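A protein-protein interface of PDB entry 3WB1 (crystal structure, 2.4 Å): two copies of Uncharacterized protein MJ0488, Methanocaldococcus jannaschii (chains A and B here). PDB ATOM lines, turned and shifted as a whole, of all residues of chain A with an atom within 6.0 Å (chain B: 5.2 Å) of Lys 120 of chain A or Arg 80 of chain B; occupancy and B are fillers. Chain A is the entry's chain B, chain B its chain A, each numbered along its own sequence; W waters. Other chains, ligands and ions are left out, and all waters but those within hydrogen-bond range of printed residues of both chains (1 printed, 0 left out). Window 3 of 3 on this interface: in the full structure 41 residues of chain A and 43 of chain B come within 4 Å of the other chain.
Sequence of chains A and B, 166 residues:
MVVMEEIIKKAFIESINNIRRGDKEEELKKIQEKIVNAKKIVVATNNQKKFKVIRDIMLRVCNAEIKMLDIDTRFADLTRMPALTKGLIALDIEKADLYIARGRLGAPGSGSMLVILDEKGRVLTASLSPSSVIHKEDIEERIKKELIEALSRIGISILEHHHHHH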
ATOM      1  N   GLU A   5     -24.941  13.707 -11.482  1.00  0.00           N
ATOM      2  CA  GLU A   5     -23.928  12.737 -11.090  1.00  0.00           C
ATOM      3  C   GLU A   5     -24.511  11.340 -10.918  1.00  0.00           C
ATOM      4  O   GLU A   5     -23.862  10.347 -11.253  1.00  0.00           O
ATOM      5  CB  GLU A   5     -23.248  13.187  -9.795  1.00  0.00           C
ATOM      6  CG  GLU A   5     -22.274  14.338  -9.981  1.00  0.00           C
ATOM      7  CD  GLU A   5     -22.966  15.663 -10.228  1.00  0.00           C
ATOM      8  OE1 GLU A   5     -24.196  15.748 -10.007  1.00  0.00           O
ATOM      9  OE2 GLU A   5     -22.285  16.620 -10.654  1.00  0.00           O
ATOM     10  N   PHE A  12     -23.021   4.754 -16.596  1.00  0.00           N
ATOM     11  CA  PHE A  12     -21.694   4.145 -16.553  1.00  0.00           C
ATOM     12  C   PHE A  12     -21.792   2.697 -16.091  1.00  0.00           C
ATOM     13  O   PHE A  12     -21.018   1.848 -16.525  1.00  0.00           O
ATOM     14  CB  PHE A  12     -20.757   4.933 -15.638  1.00  0.00           C
ATOM     15  CG  PHE A  12     -20.239   6.202 -16.256  1.00  0.00           C
ATOM     16  CD1 PHE A  12     -20.733   6.647 -17.482  1.00  0.00           C
ATOM     17  CD2 PHE A  12     -19.247   6.941 -15.627  1.00  0.00           C
ATOM     18  CE1 PHE A  12     -20.259   7.816 -18.061  1.00  0.00           C
ATOM     19  CE2 PHE A  12     -18.758   8.114 -16.202  1.00  0.00           C
ATOM     20  CZ  PHE A  12     -19.265   8.550 -17.423  1.00  0.00           C
ATOM     21  N   LYS A  34     -30.651  21.374 -17.687  1.00  0.00           N
ATOM     22  CA  LYS A  34     -29.457  22.182 -17.478  1.00  0.00           C
ATOM     23  C   LYS A  34     -29.426  23.386 -18.398  1.00  0.00           C
ATOM     24  O   LYS A  34     -29.123  24.497 -17.971  1.00  0.00           O
ATOM     25  CB  LYS A  34     -28.200  21.334 -17.682  1.00  0.00           C
ATOM     26  CG  LYS A  34     -27.861  20.438 -16.502  1.00  0.00           C
ATOM     27  CD  LYS A  34     -26.364  20.178 -16.396  1.00  0.00           C
ATOM     28  CE  LYS A  34     -25.997  19.813 -14.965  1.00  0.00           C
ATOM     29  NZ  LYS A  34     -24.532  19.606 -14.756  1.00  0.00           N
ATOM     30  N   LEU A  88     -13.190  25.167 -22.266  1.00  0.00           N
ATOM     31  CA  LEU A  88     -12.514  24.817 -21.026  1.00  0.00           C
ATOM     32  C   LEU A  88     -11.745  26.025 -20.475  1.00  0.00           C
ATOM     33  O   LEU A  88     -11.540  26.141 -19.264  1.00  0.00           O
ATOM     34  CB  LEU A  88     -11.602  23.604 -21.238  1.00  0.00           C
ATOM     35  CG  LEU A  88     -12.383  22.293 -21.476  1.00  0.00           C
ATOM     36  CD1 LEU A  88     -11.478  21.119 -21.837  1.00  0.00           C
ATOM     37  CD2 LEU A  88     -13.249  21.930 -20.263  1.00  0.00           C
ATOM     38  N   LEU A  91     -14.551  27.925 -18.834  1.00  0.00           N
ATOM     39  CA  LEU A  91     -14.877  27.184 -17.628  1.00  0.00           C
ATOM     40  C   LEU A  91     -13.888  27.520 -16.513  1.00  0.00           C
ATOM     41  O   LEU A  91     -14.265  27.640 -15.345  1.00  0.00           O
ATOM     42  CB  LEU A  91     -14.854  25.681 -17.918  1.00  0.00           C
ATOM     43  CG  LEU A  91     -14.977  24.722 -16.729  1.00  0.00           C
ATOM     44  CD1 LEU A  91     -16.315  24.858 -16.029  1.00  0.00           C
ATOM     45  CD2 LEU A  91     -14.742  23.281 -17.150  1.00  0.00           C
ATOM     46  N   TYR A  99     -21.660  26.869 -20.650  1.00  0.00           N
ATOM     47  CA  TYR A  99     -20.593  27.445 -21.466  1.00  0.00           C
ATOM     48  C   TYR A  99     -20.809  27.103 -22.941  1.00  0.00           C
ATOM     49  O   TYR A  99     -20.990  25.929 -23.292  1.00  0.00           O
ATOM     50  CB  TYR A  99     -19.223  26.929 -20.992  1.00  0.00           C
ATOM     51  CG  TYR A  99     -18.907  27.266 -19.548  1.00  0.00           C
ATOM     52  CD1 TYR A  99     -19.235  26.391 -18.522  1.00  0.00           C
ATOM     53  CD2 TYR A  99     -18.283  28.465 -19.215  1.00  0.00           C
ATOM     54  CE1 TYR A  99     -18.952  26.695 -17.202  1.00  0.00           C
ATOM     55  CE2 TYR A  99     -17.996  28.784 -17.894  1.00  0.00           C
ATOM     56  CZ  TYR A  99     -18.329  27.891 -16.894  1.00  0.00           C
ATOM     57  OH  TYR A  99     -18.050  28.184 -15.580  1.00  0.00           O
ATOM     58  N   LEU A 117     -21.183  23.314 -22.843  1.00  0.00           N
ATOM     59  CA  LEU A 117     -20.675  22.542 -21.709  1.00  0.00           C
ATOM     60  C   LEU A 117     -21.408  22.956 -20.442  1.00  0.00           C
ATOM     61  O   LEU A 117     -21.764  24.130 -20.291  1.00  0.00           O
ATOM     62  CB  LEU A 117     -19.175  22.773 -21.527  1.00  0.00           C
ATOM     63  CG  LEU A 117     -18.244  22.763 -22.742  1.00  0.00           C
ATOM     64  CD1 LEU A 117     -16.823  23.135 -22.311  1.00  0.00           C
ATOM     65  CD2 LEU A 117     -18.250  21.421 -23.444  1.00  0.00           C
ATOM     66  N   ASP A 118     -21.569  22.039 -19.495  1.00  0.00           N
ATOM     67  CA  ASP A 118     -22.175  22.418 -18.219  1.00  0.00           C
ATOM     68  C   ASP A 118     -21.096  22.927 -17.268  1.00  0.00           C
ATOM     69  O   ASP A 118     -19.961  23.167 -17.688  1.00  0.00           O
ATOM     70  CB  ASP A 118     -22.969  21.248 -17.620  1.00  0.00           C
ATOM     71  CG  ASP A 118     -22.083  20.132 -17.065  1.00  0.00           C
ATOM     72  OD1 ASP A 118     -20.842  20.148 -17.256  1.00  0.00           O
ATOM     73  OD2 ASP A 118     -22.658  19.205 -16.454  1.00  0.00           O
ATOM     74  N   GLU A 119     -21.447  23.112 -15.999  1.00  0.00           N
ATOM     75  CA  GLU A 119     -20.536  23.741 -15.042  1.00  0.00           C
ATOM     76  C   GLU A 119     -19.323  22.886 -14.686  1.00  0.00           C
ATOM     77  O   GLU A 119     -18.392  23.371 -14.048  1.00  0.00           O
ATOM     78  CB  GLU A 119     -21.292  24.105 -13.761  1.00  0.00           C
ATOM     79  CG  GLU A 119     -22.703  23.546 -13.698  1.00  0.00           C
ATOM     80  CD  GLU A 119     -22.756  22.181 -13.062  1.00  0.00           C
ATOM     81  OE1 GLU A 119     -23.495  21.318 -13.570  1.00  0.00           O
ATOM     82  OE2 GLU A 119     -22.071  21.976 -12.040  1.00  0.00           O
ATOM     83  N   LYS A 120     -19.335  21.621 -15.092  1.00  0.00           N
ATOM     84  CA  LYS A 120     -18.212  20.723 -14.833  1.00  0.00           C
ATOM     85  C   LYS A 120     -17.481  20.371 -16.125  1.00  0.00           C
ATOM     86  O   LYS A 120     -16.686  19.432 -16.161  1.00  0.00           O
ATOM     87  CB  LYS A 120     -18.691  19.452 -14.134  1.00  0.00           C
ATOM     88  CG  LYS A 120     -19.053  19.639 -12.664  1.00  0.00           C
ATOM     89  CD  LYS A 120     -19.418  18.295 -12.027  1.00  0.00           C
ATOM     90  CE  LYS A 120     -19.408  18.345 -10.503  1.00  0.00           C
ATOM     91  NZ  LYS A 120     -19.651  16.996  -9.892  1.00  0.00           N
ATOM     92  N   GLY A 121     -17.804  21.081 -17.200  1.00  0.00           N
ATOM     93  CA  GLY A 121     -17.104  20.903 -18.459  1.00  0.00           C
ATOM     94  C   GLY A 121     -17.559  19.677 -19.223  1.00  0.00           C
ATOM     95  O   GLY A 121     -16.902  19.255 -20.183  1.00  0.00           O
ATOM     96  N   ARG A 122     -18.699  19.120 -18.829  1.00  0.00           N
ATOM     97  CA  ARG A 122     -19.243  17.991 -19.559  1.00  0.00           C
ATOM     98  C   ARG A 122     -19.759  18.487 -20.896  1.00  0.00           C
ATOM     99  O   ARG A 122     -20.246  19.611 -20.996  1.00  0.00           O
ATOM    100  CB  ARG A 122     -20.375  17.302 -18.789  1.00  0.00           C
ATOM    101  CG  ARG A 122     -20.023  16.831 -17.388  1.00  0.00           C
ATOM    102  CD  ARG A 122     -21.218  16.140 -16.768  1.00  0.00           C
ATOM    103  NE  ARG A 122     -20.973  15.701 -15.398  1.00  0.00           N
ATOM    104  CZ  ARG A 122     -21.448  16.317 -14.318  1.00  0.00           C
ATOM    105  NH1 ARG A 122     -22.199  17.403 -14.445  1.00  0.00           N
ATOM    106  NH2 ARG A 122     -21.185  15.837 -13.110  1.00  0.00           N
ATOM    107  N   VAL A 123     -19.623  17.654 -21.921  1.00  0.00           N
ATOM    108  CA  VAL A 123     -20.164  17.952 -23.237  1.00  0.00           C
ATOM    109  C   VAL A 123     -21.648  17.572 -23.316  1.00  0.00           C
ATOM    110  O   VAL A 123     -21.990  16.388 -23.339  1.00  0.00           O
ATOM    111  CB  VAL A 123     -19.371  17.206 -24.335  1.00  0.00           C
ATOM    112  CG1 VAL A 123     -20.038  17.366 -25.690  1.00  0.00           C
ATOM    113  CG2 VAL A 123     -17.921  17.699 -24.367  1.00  0.00           C
ATOM    114  N   LEU B  78     -17.231   5.406 -20.477  1.00  0.00           N
ATOM    115  CA  LEU B  78     -16.984   5.854 -19.112  1.00  0.00           C
ATOM    116  C   LEU B  78     -16.256   7.189 -19.119  1.00  0.00           C
ATOM    117  O   LEU B  78     -16.104   7.837 -18.079  1.00  0.00           O
ATOM    118  CB  LEU B  78     -16.159   4.810 -18.361  1.00  0.00           C
ATOM    119  CG  LEU B  78     -16.781   3.409 -18.292  1.00  0.00           C
ATOM    120  CD1 LEU B  78     -15.844   2.415 -17.613  1.00  0.00           C
ATOM    121  CD2 LEU B  78     -18.107   3.454 -17.574  1.00  0.00           C
ATOM    122  N   THR B  79     -15.805   7.591 -20.305  1.00  0.00           N
ATOM    123  CA  THR B  79     -15.035   8.815 -20.467  1.00  0.00           C
ATOM    124  C   THR B  79     -15.939   9.933 -20.933  1.00  0.00           C
ATOM    125  O   THR B  79     -17.095   9.704 -21.300  1.00  0.00           O
ATOM    126  CB  THR B  79     -13.900   8.657 -21.485  1.00  0.00           C
ATOM    127  OG1 THR B  79     -14.462   8.458 -22.796  1.00  0.00           O
ATOM    128  CG2 THR B  79     -13.019   7.467 -21.117  1.00  0.00           C
ATOM    129  N   ARG B  80     -15.395  11.141 -20.947  1.00  0.00           N
ATOM    130  CA  ARG B  80     -16.180  12.325 -21.255  1.00  0.00           C
ATOM    131  C   ARG B  80     -16.616  12.424 -22.702  1.00  0.00           C
ATOM    132  O   ARG B  80     -17.669  12.977 -22.981  1.00  0.00           O
ATOM    133  CB  ARG B  80     -15.411  13.572 -20.849  1.00  0.00           C
ATOM    134  CG  ARG B  80     -15.305  13.676 -19.344  1.00  0.00           C
ATOM    135  CD  ARG B  80     -14.923  15.066 -18.942  1.00  0.00           C
ATOM    136  NE  ARG B  80     -15.608  15.474 -17.722  1.00  0.00           N
ATOM    137  CZ  ARG B  80     -15.533  16.697 -17.215  1.00  0.00           C
ATOM    138  NH1 ARG B  80     -14.804  17.624 -17.824  1.00  0.00           N
ATOM    139  NH2 ARG B  80     -16.190  16.997 -16.105  1.00  0.00           N
ATOM    140  N   MET B  81     -15.784  11.944 -23.620  1.00  0.00           N
ATOM    141  CA  MET B  81     -16.131  11.930 -25.036  1.00  0.00           C
ATOM    142  C   MET B  81     -15.784  10.566 -25.605  1.00  0.00           C
ATOM    143  O   MET B  81     -14.683  10.370 -26.130  1.00  0.00           O
ATOM    144  CB  MET B  81     -15.399  13.035 -25.794  1.00  0.00           C
ATOM    145  CG  MET B  81     -15.579  14.411 -25.188  1.00  0.00           C
ATOM    146  SD  MET B  81     -14.897  15.728 -26.215  1.00  0.00           S
ATOM    147  CE  MET B  81     -15.981  15.647 -27.643  1.00  0.00           C
ATOM    148  N   PRO B  82     -16.733   9.622 -25.516  1.00  0.00           N
ATOM    149  CA  PRO B  82     -16.557   8.204 -25.862  1.00  0.00           C
ATOM    150  C   PRO B  82     -16.046   7.975 -27.287  1.00  0.00           C
ATOM    151  O   PRO B  82     -15.207   7.093 -27.498  1.00  0.00           O
ATOM    152  CB  PRO B  82     -17.968   7.632 -25.694  1.00  0.00           C
ATOM    153  CG  PRO B  82     -18.616   8.535 -24.672  1.00  0.00           C
ATOM    154  CD  PRO B  82     -18.083   9.900 -24.988  1.00  0.00           C
ATOM    155  N   LEU B 105     -21.190  11.188 -28.090  1.00  0.00           N
ATOM    156  CA  LEU B 105     -20.517  12.480 -28.182  1.00  0.00           C
ATOM    157  C   LEU B 105     -19.852  12.831 -26.869  1.00  0.00           C
ATOM    158  O   LEU B 105     -18.631  13.024 -26.795  1.00  0.00           O
ATOM    159  CB  LEU B 105     -21.535  13.574 -28.547  1.00  0.00           C
ATOM    160  CG  LEU B 105     -21.185  14.961 -29.121  1.00  0.00           C
ATOM    161  CD1 LEU B 105     -22.189  16.012 -28.660  1.00  0.00           C
ATOM    162  CD2 LEU B 105     -19.769  15.414 -28.820  1.00  0.00           C
ATOM    163  N   GLY B 106     -20.680  12.974 -25.841  1.00  0.00           N
ATOM    164  CA  GLY B 106     -20.202  13.421 -24.554  1.00  0.00           C
ATOM    165  C   GLY B 106     -20.899  12.744 -23.395  1.00  0.00           C
ATOM    166  O   GLY B 106     -20.827  11.519 -23.227  1.00  0.00           O
ATOM    167  N   ALA B 107     -21.585  13.546 -22.590  1.00  0.00           N
ATOM    168  CA  ALA B 107     -22.313  13.012 -21.449  1.00  0.00           C
ATOM    169  C   ALA B 107     -23.453  12.130 -21.945  1.00  0.00           C
ATOM    170  O   ALA B 107     -23.905  12.278 -23.089  1.00  0.00           O
ATOM    171  CB  ALA B 107     -22.841  14.146 -20.576  1.00  0.00           C
HETATM  172  O   HOH W   1     -18.977  14.813 -21.333  1.00  0.00           O
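Of the 13 printed residues of chain A, 4 touch a printed residue of chain B.
Hydrophobic or aromatic side chains of chain A that line the printed part of chain B: Phe 12 and Val 123.
Along chain A the printed residues that touch a printed residue of chain B span positions 12 to 123.
The side-chain carboxylate of Asp 118 of chain A sits at hydrogen-bond distance from the backbone NH of Lys 120 of chain A.
NZ of Lys 120 of chain A is in salt-bridge range of OE2 of Glu 5 of chain A, at 2.8 Å.
N of Gly 121 of chain A sits at hydrogen-bond distance from OD1 of Asp 118 of chain A, 3.2 Å away.
Among the printed residues, pairs that only touch across the chains: Phe 12 of chain A with Leu 78 of chain B (3.3 Å), Gly 121 of chain A with Arg 80 of chain B (3.6 Å), Val 123 of chain A with Gly 106 of chain B (3.7 Å) and Val 123 of chain A with Leu 105 of chain B (3.7 Å).
Water W1 lies within hydrogen-bond range of the backbone carbonyl oxygen (O) of Arg 80 of chain B (2.8 Å), the backbone NH (N) of Val 123 of chain A (3.0 Å) and the backbone NH (N) of Ala 107 of chain B (3.2 Å).
No position is printed for both chains.
The guanidinium group (NH2) of Arg 80 of chain B lies within hydrogen-bond range of the backbone carbonyl oxygen (O) of Lys 120 of chain A, at 2.5 Å.
The backbone NH (N) of Ala 107 of chain B sits at hydrogen-bond distance from the backbone carbonyl oxygen (O) of Val 123 of chain A (3.0 Å).
Lys 120 of chain A touches just one residue of chain B: Arg 80 (2.5 Å).
Arg 80 of chain B touches just these residues of chain A: Lys 120 and Gly 121.
Of the printed residues of chain A, Leu 78 of chain B touches Phe 12 (3.3 Å).
Printed residues of chain A within 4 Å of Leu 105 of chain B: Val 123.
Of the printed residues of chain B, Val 123 of chain A touches Leu 105, Gly 106 and Ala 107.
Printed residues of chain A within 4 Å of Gly 106 of chain B: Val 123.
Leu 91 of chain A touches none of the printed residues of chain B.
Glu 119 of chain A touches none of the printed residues of chain B.
The nearest residue of chain A that does not touch Arg 80 of chain B is Arg 122 of chain A (4.05 Å).
The nearest printed residue of chain A that does not touch Gly 106 of chain B is Arg 122 of chain A (6.3 Å).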
